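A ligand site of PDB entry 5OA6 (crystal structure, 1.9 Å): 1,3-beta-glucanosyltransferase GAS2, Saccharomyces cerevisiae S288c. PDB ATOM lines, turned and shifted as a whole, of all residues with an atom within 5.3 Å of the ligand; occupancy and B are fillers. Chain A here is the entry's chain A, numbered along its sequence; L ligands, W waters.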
ATOM      1  N   GLN A  60      -1.740 -18.324  -2.828  1.00  0.00           N
ATOM      2  CA  GLN A  60      -0.403 -18.463  -3.368  1.00  0.00           C
ATOM      3  C   GLN A  60      -0.436 -19.206  -4.694  1.00  0.00           C
ATOM      4  O   GLN A  60      -0.990 -20.307  -4.784  1.00  0.00           O
ATOM      5  CB  GLN A  60       0.472 -19.245  -2.391  1.00  0.00           C
ATOM      6  CG  GLN A  60       1.954 -19.285  -2.770  1.00  0.00           C
ATOM      7  CD  GLN A  60       2.670 -17.985  -2.522  1.00  0.00           C
ATOM      8  OE1 GLN A  60       2.516 -17.375  -1.478  1.00  0.00           O
ATOM      9  NE2 GLN A  60       3.505 -17.551  -3.479  1.00  0.00           N
ATOM     10  N   GLN A  62       1.681 -20.970  -7.873  1.00  0.00           N
ATOM     11  CA  GLN A  62       2.978 -21.626  -8.111  1.00  0.00           C
ATOM     12  C   GLN A  62       3.132 -22.030  -9.569  1.00  0.00           C
ATOM     13  O   GLN A  62       2.144 -22.311 -10.251  1.00  0.00           O
ATOM     14  CB  GLN A  62       3.177 -22.821  -7.164  1.00  0.00           C
ATOM     15  CG  GLN A  62       2.522 -24.122  -7.590  1.00  0.00           C
ATOM     16  CD  GLN A  62       2.333 -25.111  -6.440  1.00  0.00           C
ATOM     17  OE1 GLN A  62       2.964 -24.993  -5.379  1.00  0.00           O
ATOM     18  NE2 GLN A  62       1.472 -26.106  -6.646  1.00  0.00           N
ATOM     19  N   TYR A 107       2.685 -17.648   1.268  1.00  0.00           N
ATOM     20  CA  TYR A 107       3.872 -18.478   1.543  1.00  0.00           C
ATOM     21  C   TYR A 107       5.157 -17.842   1.037  1.00  0.00           C
ATOM     22  O   TYR A 107       6.239 -18.171   1.544  1.00  0.00           O
ATOM     23  CB  TYR A 107       3.696 -19.882   0.947  1.00  0.00           C
ATOM     24  CG  TYR A 107       2.593 -20.672   1.605  1.00  0.00           C
ATOM     25  CD1 TYR A 107       1.274 -20.562   1.170  1.00  0.00           C
ATOM     26  CD2 TYR A 107       2.854 -21.552   2.676  1.00  0.00           C
ATOM     27  CE1 TYR A 107       0.258 -21.276   1.774  1.00  0.00           C
ATOM     28  CE2 TYR A 107       1.837 -22.290   3.275  1.00  0.00           C
ATOM     29  CZ  TYR A 107       0.530 -22.151   2.820  1.00  0.00           C
ATOM     30  OH  TYR A 107      -0.520 -22.858   3.387  1.00  0.00           O
ATOM     31  N   ALA A 108       5.067 -16.945   0.063  1.00  0.00           N
ATOM     32  CA  ALA A 108       6.255 -16.350  -0.529  1.00  0.00           C
ATOM     33  C   ALA A 108       5.947 -15.041  -1.231  1.00  0.00           C
ATOM     34  O   ALA A 108       5.062 -15.008  -2.080  1.00  0.00           O
ATOM     35  CB  ALA A 108       6.897 -17.333  -1.490  1.00  0.00           C
ATOM     36  N   ASP A 132       4.728 -16.189   5.461  1.00  0.00           N
ATOM     37  CA  ASP A 132       5.990 -16.894   5.711  1.00  0.00           C
ATOM     38  C   ASP A 132       7.171 -16.013   5.292  1.00  0.00           C
ATOM     39  O   ASP A 132       7.085 -15.271   4.309  1.00  0.00           O
ATOM     40  CB  ASP A 132       6.047 -18.220   4.953  1.00  0.00           C
ATOM     41  CG  ASP A 132       4.946 -19.179   5.392  1.00  0.00           C
ATOM     42  OD1 ASP A 132       3.771 -18.961   5.031  1.00  0.00           O
ATOM     43  OD2 ASP A 132       5.255 -20.159   6.113  1.00  0.00           O
ATOM     44  N   SER A 134      10.254 -17.349   4.669  1.00  0.00           N
ATOM     45  CA  SER A 134      11.084 -18.162   3.808  1.00  0.00           C
ATOM     46  C   SER A 134      10.534 -18.255   2.384  1.00  0.00           C
ATOM     47  O   SER A 134       9.440 -17.756   2.061  1.00  0.00           O
ATOM     48  CB  SER A 134      11.241 -19.551   4.447  1.00  0.00           C
ATOM     49  OG  SER A 134       9.965 -20.158   4.655  1.00  0.00           O
ATOM     50  N   GLU A 135      11.300 -18.891   1.503  1.00  0.00           N
ATOM     51  CA  GLU A 135      10.793 -19.285   0.190  1.00  0.00           C
ATOM     52  C   GLU A 135      11.466 -20.620  -0.154  1.00  0.00           C
ATOM     53  O   GLU A 135      12.453 -20.975   0.479  1.00  0.00           O
ATOM     54  CB  GLU A 135      11.034 -18.162  -0.851  1.00  0.00           C
ATOM     55  CG  GLU A 135      12.485 -17.752  -1.086  1.00  0.00           C
ATOM     56  CD  GLU A 135      13.102 -18.357  -2.338  1.00  0.00           C
ATOM     57  OE1 GLU A 135      12.677 -19.431  -2.815  1.00  0.00           O
ATOM     58  OE2 GLU A 135      14.043 -17.720  -2.852  1.00  0.00           O
ATOM     59  N   PRO A 136      10.909 -21.375  -1.127  1.00  0.00           N
ATOM     60  CA  PRO A 136      11.386 -22.756  -1.293  1.00  0.00           C
ATOM     61  C   PRO A 136      12.893 -22.937  -1.423  1.00  0.00           C
ATOM     62  O   PRO A 136      13.431 -23.918  -0.915  1.00  0.00           O
ATOM     63  CB  PRO A 136      10.664 -23.241  -2.566  1.00  0.00           C
ATOM     64  CG  PRO A 136       9.475 -22.363  -2.681  1.00  0.00           C
ATOM     65  CD  PRO A 136       9.854 -21.038  -2.088  1.00  0.00           C
ATOM     66  N   ASP A 137      13.569 -21.977  -2.071  1.00  0.00           N
ATOM     67  CA  ASP A 137      15.009 -22.006  -2.269  1.00  0.00           C
ATOM     68  C   ASP A 137      15.815 -21.350  -1.157  1.00  0.00           C
ATOM     69  O   ASP A 137      17.030 -21.452  -1.164  1.00  0.00           O
ATOM     70  CB  ASP A 137      15.395 -21.359  -3.613  1.00  0.00           C
ATOM     71  CG  ASP A 137      14.857 -22.132  -4.820  1.00  0.00           C
ATOM     72  OD1 ASP A 137      14.648 -23.355  -4.724  1.00  0.00           O
ATOM     73  OD2 ASP A 137      14.647 -21.493  -5.866  1.00  0.00           O
ATOM     74  N   SER A 139      15.176 -21.507   2.730  1.00  0.00           N
ATOM     75  CA  SER A 139      14.436 -22.003   3.876  1.00  0.00           C
ATOM     76  C   SER A 139      15.427 -22.754   4.738  1.00  0.00           C
ATOM     77  O   SER A 139      16.466 -23.196   4.232  1.00  0.00           O
ATOM     78  CB  SER A 139      13.392 -23.005   3.409  1.00  0.00           C
ATOM     79  OG  SER A 139      12.249 -22.371   2.880  1.00  0.00           O
ATOM     80  N   ILE A 140      15.081 -22.962   6.009  1.00  0.00           N
ATOM     81  CA  ILE A 140      15.891 -23.866   6.849  1.00  0.00           C
ATOM     82  C   ILE A 140      15.694 -25.288   6.311  1.00  0.00           C
ATOM     83  O   ILE A 140      14.575 -25.778   6.252  1.00  0.00           O
ATOM     84  CB  ILE A 140      15.509 -23.754   8.343  1.00  0.00           C
ATOM     85  CG1 ILE A 140      15.788 -22.340   8.878  1.00  0.00           C
ATOM     86  CG2 ILE A 140      16.257 -24.811   9.168  1.00  0.00           C
ATOM     87  CD1 ILE A 140      15.143 -22.046  10.214  1.00  0.00           C
ATOM     88  N   ASN A 141      16.782 -25.922   5.871  1.00  0.00           N
ATOM     89  CA  ASN A 141      16.737 -27.230   5.197  1.00  0.00           C
ATOM     90  C   ASN A 141      16.611 -28.312   6.252  1.00  0.00           C
ATOM     91  O   ASN A 141      17.547 -28.551   7.022  1.00  0.00           O
ATOM     92  CB  ASN A 141      18.024 -27.437   4.389  1.00  0.00           C
ATOM     93  CG  ASN A 141      18.019 -28.716   3.541  1.00  0.00           C
ATOM     94  OD1 ASN A 141      17.166 -29.602   3.689  1.00  0.00           O
ATOM     95  ND2 ASN A 141      18.983 -28.810   2.627  1.00  0.00           N
ATOM     96  N   ARG A 142      15.481 -28.984   6.298  1.00  0.00           N
ATOM     97  CA  ARG A 142      15.235 -29.971   7.358  1.00  0.00           C
ATOM     98  C   ARG A 142      16.193 -31.186   7.259  1.00  0.00           C
ATOM     99  O   ARG A 142      16.409 -31.869   8.227  1.00  0.00           O
ATOM    100  CB  ARG A 142      13.785 -30.417   7.365  1.00  0.00           C
ATOM    101  CG  ARG A 142      13.326 -31.257   6.187  1.00  0.00           C
ATOM    102  CD  ARG A 142      11.904 -31.784   6.410  1.00  0.00           C
ATOM    103  NE  ARG A 142      10.828 -30.788   6.255  1.00  0.00           N
ATOM    104  CZ  ARG A 142      10.291 -30.404   5.104  1.00  0.00           C
ATOM    105  NH1 ARG A 142      10.750 -30.865   3.923  1.00  0.00           N
ATOM    106  NH2 ARG A 142       9.295 -29.535   5.099  1.00  0.00           N
ATOM    107  N   GLU A 143      16.755 -31.405   6.077  1.00  0.00           N
ATOM    108  CA  GLU A 143      17.703 -32.515   5.815  1.00  0.00           C
ATOM    109  C   GLU A 143      19.133 -32.151   6.186  1.00  0.00           C
ATOM    110  O   GLU A 143      19.996 -33.039   6.332  1.00  0.00           O
ATOM    111  CB  GLU A 143      17.657 -32.866   4.326  1.00  0.00           C
ATOM    112  CG  GLU A 143      16.256 -33.161   3.777  1.00  0.00           C
ATOM    113  CD  GLU A 143      15.617 -34.366   4.451  1.00  0.00           C
ATOM    114  OE1 GLU A 143      16.368 -35.246   4.928  1.00  0.00           O
ATOM    115  OE2 GLU A 143      14.366 -34.450   4.487  1.00  0.00           O
ATOM    116  N   ASN A 175       7.952 -23.439   8.366  1.00  0.00           N
ATOM    117  CA  ASN A 175       6.761 -24.218   8.034  1.00  0.00           C
ATOM    118  C   ASN A 175       7.162 -25.686   7.925  1.00  0.00           C
ATOM    119  O   ASN A 175       7.899 -26.056   7.019  1.00  0.00           O
ATOM    120  CB  ASN A 175       6.144 -23.741   6.717  1.00  0.00           C
ATOM    121  CG  ASN A 175       4.906 -24.521   6.331  1.00  0.00           C
ATOM    122  OD1 ASN A 175       3.934 -24.523   7.062  1.00  0.00           O
ATOM    123  ND2 ASN A 175       4.942 -25.205   5.193  1.00  0.00           N
ATOM    124  N   GLU A 176       6.698 -26.491   8.880  1.00  0.00           N
ATOM    125  CA  GLU A 176       6.903 -27.938   8.884  1.00  0.00           C
ATOM    126  C   GLU A 176       8.363 -28.290   8.678  1.00  0.00           C
ATOM    127  O   GLU A 176       8.702 -29.084   7.788  1.00  0.00           O
ATOM    128  CB  GLU A 176       6.049 -28.596   7.797  1.00  0.00           C
ATOM    129  CG  GLU A 176       4.602 -28.199   7.837  1.00  0.00           C
ATOM    130  CD  GLU A 176       3.750 -29.038   6.932  1.00  0.00           C
ATOM    131  OE1 GLU A 176       4.308 -29.746   6.050  1.00  0.00           O
ATOM    132  OE2 GLU A 176       2.521 -29.008   7.123  1.00  0.00           O
ATOM    133  N   VAL A 177       9.245 -27.669   9.460  1.00  0.00           N
ATOM    134  CA  VAL A 177      10.689 -27.873   9.288  1.00  0.00           C
ATOM    135  C   VAL A 177      11.013 -29.280   9.824  1.00  0.00           C
ATOM    136  O   VAL A 177      11.191 -30.187   9.033  1.00  0.00           O
ATOM    137  CB  VAL A 177      11.543 -26.751   9.908  1.00  0.00           C
ATOM    138  CG1 VAL A 177      13.011 -26.943   9.567  1.00  0.00           C
ATOM    139  CG2 VAL A 177      11.072 -25.395   9.373  1.00  0.00           C
ATOM    140  N   TYR A 244      -5.387 -31.520   9.052  1.00  0.00           N
ATOM    141  CA  TYR A 244      -6.205 -32.214   8.045  1.00  0.00           C
ATOM    142  C   TYR A 244      -6.961 -33.448   8.595  1.00  0.00           C
ATOM    143  O   TYR A 244      -7.397 -34.307   7.820  1.00  0.00           O
ATOM    144  CB  TYR A 244      -5.315 -32.617   6.868  1.00  0.00           C
ATOM    145  CG  TYR A 244      -4.794 -31.434   6.104  1.00  0.00           C
ATOM    146  CD1 TYR A 244      -3.604 -30.802   6.473  1.00  0.00           C
ATOM    147  CD2 TYR A 244      -5.500 -30.916   5.033  1.00  0.00           C
ATOM    148  CE1 TYR A 244      -3.122 -29.707   5.767  1.00  0.00           C
ATOM    149  CE2 TYR A 244      -5.034 -29.818   4.320  1.00  0.00           C
ATOM    150  CZ  TYR A 244      -3.854 -29.207   4.688  1.00  0.00           C
ATOM    151  OH  TYR A 244      -3.396 -28.129   3.974  1.00  0.00           O
ATOM    152  N   GLU A 275      -3.498 -24.258   8.257  1.00  0.00           N
ATOM    153  CA  GLU A 275      -4.164 -24.842   7.098  1.00  0.00           C
ATOM    154  C   GLU A 275      -5.248 -25.767   7.600  1.00  0.00           C
ATOM    155  O   GLU A 275      -5.082 -26.407   8.658  1.00  0.00           O
ATOM    156  CB  GLU A 275      -3.175 -25.674   6.243  1.00  0.00           C
ATOM    157  CG  GLU A 275      -2.074 -24.886   5.543  1.00  0.00           C
ATOM    158  CD  GLU A 275      -0.977 -25.763   4.925  1.00  0.00           C
ATOM    159  OE1 GLU A 275      -1.129 -27.011   4.891  1.00  0.00           O
ATOM    160  OE2 GLU A 275       0.032 -25.179   4.455  1.00  0.00           O
ATOM    161  N   CYS A 278      -9.216 -31.067   4.443  1.00  0.00           N
ATOM    162  CA  CYS A 278      -8.975 -32.423   3.913  1.00  0.00           C
ATOM    163  C   CYS A 278      -9.935 -32.647   2.765  1.00  0.00           C
ATOM    164  O   CYS A 278     -11.119 -32.309   2.880  1.00  0.00           O
ATOM    165  CB  CYS A 278      -9.210 -33.481   4.980  1.00  0.00           C
ATOM    166  SG  CYS A 278      -9.185 -35.193   4.389  1.00  0.00           S
ATOM    167  N   TYR A 307      -7.128 -24.383   3.085  1.00  0.00           N
ATOM    168  CA  TYR A 307      -6.120 -24.586   2.055  1.00  0.00           C
ATOM    169  C   TYR A 307      -6.842 -25.167   0.847  1.00  0.00           C
ATOM    170  O   TYR A 307      -7.320 -26.287   0.947  1.00  0.00           O
ATOM    171  CB  TYR A 307      -5.041 -25.564   2.557  1.00  0.00           C
ATOM    172  CG  TYR A 307      -3.944 -25.739   1.550  1.00  0.00           C
ATOM    173  CD1 TYR A 307      -2.846 -24.887   1.531  1.00  0.00           C
ATOM    174  CD2 TYR A 307      -4.016 -26.746   0.575  1.00  0.00           C
ATOM    175  CE1 TYR A 307      -1.852 -25.022   0.573  1.00  0.00           C
ATOM    176  CE2 TYR A 307      -3.011 -26.891  -0.380  1.00  0.00           C
ATOM    177  CZ  TYR A 307      -1.941 -26.041  -0.381  1.00  0.00           C
ATOM    178  OH  TYR A 307      -0.948 -26.192  -1.311  1.00  0.00           O
ATOM    179  N   MET A 308      -6.971 -24.467  -0.292  1.00  0.00           N
ATOM    180  CA  MET A 308      -6.512 -23.092  -0.532  1.00  0.00           C
ATOM    181  C   MET A 308      -7.344 -22.446  -1.647  1.00  0.00           C
ATOM    182  O   MET A 308      -8.285 -23.051  -2.159  1.00  0.00           O
ATOM    183  CB  MET A 308      -5.026 -23.084  -0.900  1.00  0.00           C
ATOM    184  CG  MET A 308      -4.678 -23.721  -2.234  1.00  0.00           C
ATOM    185  SD  MET A 308      -3.016 -23.294  -2.782  1.00  0.00           S
ATOM    186  CE  MET A 308      -3.282 -21.579  -3.199  1.00  0.00           C
ATOM    187  N   GLU A 312      -4.568 -26.100  -8.263  1.00  0.00           N
ATOM    188  CA  GLU A 312      -3.316 -26.370  -8.966  1.00  0.00           C
ATOM    189  C   GLU A 312      -3.027 -27.884  -9.081  1.00  0.00           C
ATOM    190  O   GLU A 312      -1.884 -28.309  -9.044  1.00  0.00           O
ATOM    191  CB  GLU A 312      -2.152 -25.669  -8.251  1.00  0.00           C
ATOM    192  CG  GLU A 312      -2.373 -24.173  -8.077  1.00  0.00           C
ATOM    193  CD  GLU A 312      -1.150 -23.466  -7.549  1.00  0.00           C
ATOM    194  OE1 GLU A 312      -0.783 -22.431  -8.139  1.00  0.00           O
ATOM    195  OE2 GLU A 312      -0.566 -23.954  -6.551  1.00  0.00           O
ATOM    196  N   ASN A 314      -3.499 -30.384  -7.108  1.00  0.00           N
ATOM    197  CA  ASN A 314      -3.541 -31.191  -5.890  1.00  0.00           C
ATOM    198  C   ASN A 314      -4.999 -31.276  -5.408  1.00  0.00           C
ATOM    199  O   ASN A 314      -5.264 -31.898  -4.385  1.00  0.00           O
ATOM    200  CB  ASN A 314      -2.538 -30.683  -4.824  1.00  0.00           C
ATOM    201  CG  ASN A 314      -2.637 -29.179  -4.545  1.00  0.00           C
ATOM    202  OD1 ASN A 314      -3.511 -28.481  -5.072  1.00  0.00           O
ATOM    203  ND2 ASN A 314      -1.737 -28.669  -3.700  1.00  0.00           N
ATOM    204  N   TYR A 316      -7.088 -29.001  -4.237  1.00  0.00           N
ATOM    205  CA  TYR A 316      -7.334 -28.250  -2.997  1.00  0.00           C
ATOM    206  C   TYR A 316      -7.904 -26.834  -3.214  1.00  0.00           C
ATOM    207  O   TYR A 316      -8.161 -26.134  -2.253  1.00  0.00           O
ATOM    208  CB  TYR A 316      -6.051 -28.135  -2.177  1.00  0.00           C
ATOM    209  CG  TYR A 316      -5.695 -29.397  -1.451  1.00  0.00           C
ATOM    210  CD1 TYR A 316      -6.378 -29.771  -0.300  1.00  0.00           C
ATOM    211  CD2 TYR A 316      -4.699 -30.239  -1.917  1.00  0.00           C
ATOM    212  CE1 TYR A 316      -6.045 -30.933   0.383  1.00  0.00           C
ATOM    213  CE2 TYR A 316      -4.364 -31.415  -1.260  1.00  0.00           C
ATOM    214  CZ  TYR A 316      -5.043 -31.752  -0.107  1.00  0.00           C
ATOM    215  OH  TYR A 316      -4.719 -32.913   0.541  1.00  0.00           O
HETATM  216  C1  LIG L   1       3.467 -24.023  -0.603  1.00  0.00           C
HETATM  217  C2  LIG L   1       1.975 -23.932  -0.273  1.00  0.00           C
HETATM  218  C3  LIG L   1       1.024 -23.465  -1.355  1.00  0.00           C
HETATM  219  C4  LIG L   1       4.165 -24.641   0.600  1.00  0.00           C
HETATM  220  C5  LIG L   1       0.006 -32.556   4.313  1.00  0.00           C
HETATM  221  C6  LIG L   1       0.461 -33.446   5.280  1.00  0.00           C
HETATM  222  C7  LIG L   1      -0.356 -34.489   5.687  1.00  0.00           C
HETATM  223  C8  LIG L   1      -1.622 -34.634   5.131  1.00  0.00           C
HETATM  224  C9  LIG L   1      -2.408 -35.697   5.579  1.00  0.00           C
HETATM  225  C10 LIG L   1      -3.684 -35.908   5.051  1.00  0.00           C
HETATM  226  C11 LIG L   1      -4.170 -35.043   4.072  1.00  0.00           C
HETATM  227  C12 LIG L   1      -3.380 -33.966   3.621  1.00  0.00           C
HETATM  228  C13 LIG L   1      -2.095 -33.739   4.133  1.00  0.00           C
HETATM  229  N1  LIG L   1      -1.300 -32.701   3.715  1.00  0.00           N
HETATM  230  C14 LIG L   1      -1.790 -31.752   2.674  1.00  0.00           C
HETATM  231  C15 LIG L   1      -0.678 -30.767   2.294  1.00  0.00           C
HETATM  232  C16 LIG L   1      -1.291 -29.663   1.470  1.00  0.00           C
HETATM  233  C17 LIG L   1      -0.100 -28.744   1.119  1.00  0.00           C
HETATM  234  C18 LIG L   1       0.170 -27.531   1.596  1.00  0.00           C
HETATM  235  N2  LIG L   1       0.862 -29.067   0.255  1.00  0.00           N
HETATM  236  N3  LIG L   1       1.650 -28.134   0.191  1.00  0.00           N
HETATM  237  N4  LIG L   1       1.314 -27.185   0.983  1.00  0.00           N
HETATM  238  C19 LIG L   1       2.056 -25.900   1.105  1.00  0.00           C
HETATM  239  C20 LIG L   1       3.573 -26.023   0.913  1.00  0.00           C
HETATM  240  O1  LIG L   1       4.131 -26.528   2.118  1.00  0.00           O
HETATM  241  O2  LIG L   1       1.485 -25.241  -0.007  1.00  0.00           O
HETATM  242  O3  LIG L   1       1.759 -23.182  -2.543  1.00  0.00           O
HETATM  243  O4  LIG L   1       4.042 -22.733  -0.882  1.00  0.00           O
HETATM  244  O5  LIG L   1       5.547 -24.789   0.253  1.00  0.00           O
HETATM  245  C21 LIG L   1       6.471 -24.435   1.280  1.00  0.00           C
HETATM  246  C22 LIG L   1       7.873 -24.849   0.827  1.00  0.00           C
HETATM  247  O6  LIG L   1       7.906 -26.264   0.680  1.00  0.00           O
HETATM  248  O7  LIG L   1       6.439 -23.041   1.462  1.00  0.00           O
HETATM  249  C23 LIG L   1       7.303 -22.587   2.523  1.00  0.00           C
HETATM  250  C24 LIG L   1       6.978 -21.101   2.639  1.00  0.00           C
HETATM  251  O8  LIG L   1       7.673 -20.388   1.594  1.00  0.00           O
HETATM  252  C25 LIG L   1       8.764 -22.924   2.170  1.00  0.00           C
HETATM  253  O9  LIG L   1       9.599 -22.621   3.287  1.00  0.00           O
HETATM  254  C26 LIG L   1       8.881 -24.415   1.870  1.00  0.00           C
HETATM  255  O10 LIG L   1      10.217 -24.674   1.390  1.00  0.00           O
HETATM  256  C27 LIG L   1      10.823 -25.829   2.001  1.00  0.00           C
HETATM  257  O11 LIG L   1      10.948 -25.650   3.432  1.00  0.00           O
HETATM  258  C28 LIG L   1      11.468 -26.832   4.085  1.00  0.00           C
HETATM  259  C29 LIG L   1      11.517 -26.730   5.607  1.00  0.00           C
HETATM  260  O12 LIG L   1      12.004 -25.414   5.881  1.00  0.00           O
HETATM  261  C30 LIG L   1      12.915 -27.104   3.550  1.00  0.00           C
HETATM  262  O13 LIG L   1      13.423 -28.349   4.087  1.00  0.00           O
HETATM  263  C31 LIG L   1      12.940 -27.181   2.028  1.00  0.00           C
HETATM  264  O14 LIG L   1      14.313 -27.162   1.556  1.00  0.00           O
HETATM  265  C32 LIG L   1      12.225 -25.976   1.410  1.00  0.00           C
HETATM  266  O15 LIG L   1      12.154 -26.156   0.003  1.00  0.00           O
HETATM  267  O   HOH W   1       9.763 -26.981  -1.261  1.00  0.00           O
HETATM  268  O   HOH W   2       0.386 -22.548  -4.591  1.00  0.00           O
HETATM  269  O   HOH W   3       2.377 -26.506   4.250  1.00  0.00           O
HETATM  270  O   HOH W   4      -6.308 -36.451   6.911  1.00  0.00           O
HETATM  271  O   HOH W   5      10.205 -23.292   6.270  1.00  0.00           O
HETATM  272  O   HOH W   6      13.779 -30.439   2.396  1.00  0.00           O
HETATM  273  O   HOH W   7      -1.459 -33.942   8.481  1.00  0.00           O
HETATM  274  O   HOH W   8      -6.624 -34.063   2.156  1.00  0.00           O
HETATM  275  O   HOH W   9       7.304 -26.127   4.429  1.00  0.00           O
HETATM  276  O   HOH W  10       2.064 -26.195  -3.070  1.00  0.00           O
HETATM  277  O   HOH W  11      15.175 -27.866  -0.860  1.00  0.00           O
HETATM  278  O   HOH W  12       0.659 -28.978   4.874  1.00  0.00           O
HETATM  279  O   HOH W  13       3.854 -22.296  -3.687  1.00  0.00           O
HETATM  280  O   HOH W  14       6.490 -21.415  -1.116  1.00  0.00           O
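Water W2 lies within hydrogen-bond range of an oxygen (O3) of the ligand (2.5 Å), the side-chain carboxylate of Glu 312 (2.6 Å) and the backbone carbonyl oxygen of Gln 60 (2.6 Å).
Water W13 bridges an oxygen (O3) of the ligand (2.5 Å) and the side-chain amide oxygen of Gln 62 (3.3 Å).
Water W3 lies within hydrogen-bond range of the side-chain carboxylate of Glu 275 (2.7 Å), an oxygen (O1) of the ligand (2.8 Å) and the side-chain amide nitrogen of Asn 175 (3.0 Å).
Water W5 lies within hydrogen-bond range of O12 of the ligand and N of Asn 175.
Water W10 lies within hydrogen-bond range of OE1 of Gln 62 (2.8 Å), O3 of the ligand (3.1 Å) and OH of Tyr 307 (3.5 Å).
Water W12 bridges the side-chain carboxylate of Glu 275 and the side-chain carboxylate of Glu 176.
OE2 of Glu 275 is in hydrogen-bond range of OH of Tyr 107.
OE1 of Gln 60 sits at hydrogen-bond distance from N of Tyr 107 (2.8 Å).
OG of Ser 139 sits at hydrogen-bond distance from O of Glu 135.
NE of Arg 142 is in hydrogen-bond range of O of Val 177 (2.9 Å).
The backbone carbonyl oxygen (O) of Glu 176 sits at hydrogen-bond distance from the guanidinium group (NH2) of Arg 142, 2.8 Å away.
The backbone NH (N) of Gln 62 sits at hydrogen-bond distance from the side-chain carboxylate (OE1) of Glu 312, at 2.9 Å.
The side-chain carboxylate (OE1) of Glu 275 lies within hydrogen-bond range of the side-chain hydroxyl (OH) of Tyr 244, 2.7 Å away.
The side-chain amide oxygen of Gln 60 sits at hydrogen-bond distance from the backbone NH of Ala 108, at 3.0 Å.
O of Ile 140 is in hydrogen-bond range of O12 of the ligand.
An oxygen (O8) of the ligand is in hydrogen-bond range of the backbone carbonyl oxygen (O) of Tyr 107, 2.6 Å away.
The side-chain hydroxyl (OG) of Ser 139 lies within hydrogen-bond range of an oxygen (O9) of the ligand.
The backbone carbonyl oxygen (O) of Pro 136 lies within hydrogen-bond range of an oxygen (O15) of the ligand (2.7 Å).
An oxygen (O8) of the ligand lies within hydrogen-bond range of the backbone carbonyl oxygen (O) of Ser 134, 3.2 Å away.
OG of Ser 134 is in hydrogen-bond range of O9 of the ligand (2.8 Å).
OH of Tyr 307 is in hydrogen-bond range of O2 of the ligand (2.9 Å).
N of Arg 142 lies within hydrogen-bond range of O13 of the ligand (3.1 Å).
ND2 of Asn 175 is in hydrogen-bond range of O1 of the ligand (3.4 Å).
Gln 60 touches the ligand.
OE1 of Gln 62 touches O3 of the ligand (3.6 Å).
CB of Asp 132 touches C24 of the ligand, at 3.8 Å.
CA of Glu 135 touches O8 of the ligand, 3.6 Å away.
CA of Asn 141 touches O13 of the ligand (3.7 Å).
Val 177 touches the ligand (CG2 to O12, 3.6 Å).
Tyr 244 touches the ligand.
OE1 of Glu 275 touches C18 of the ligand (3.6 Å).
Tyr 316 touches the ligand (OH to C12, 3.5 Å).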
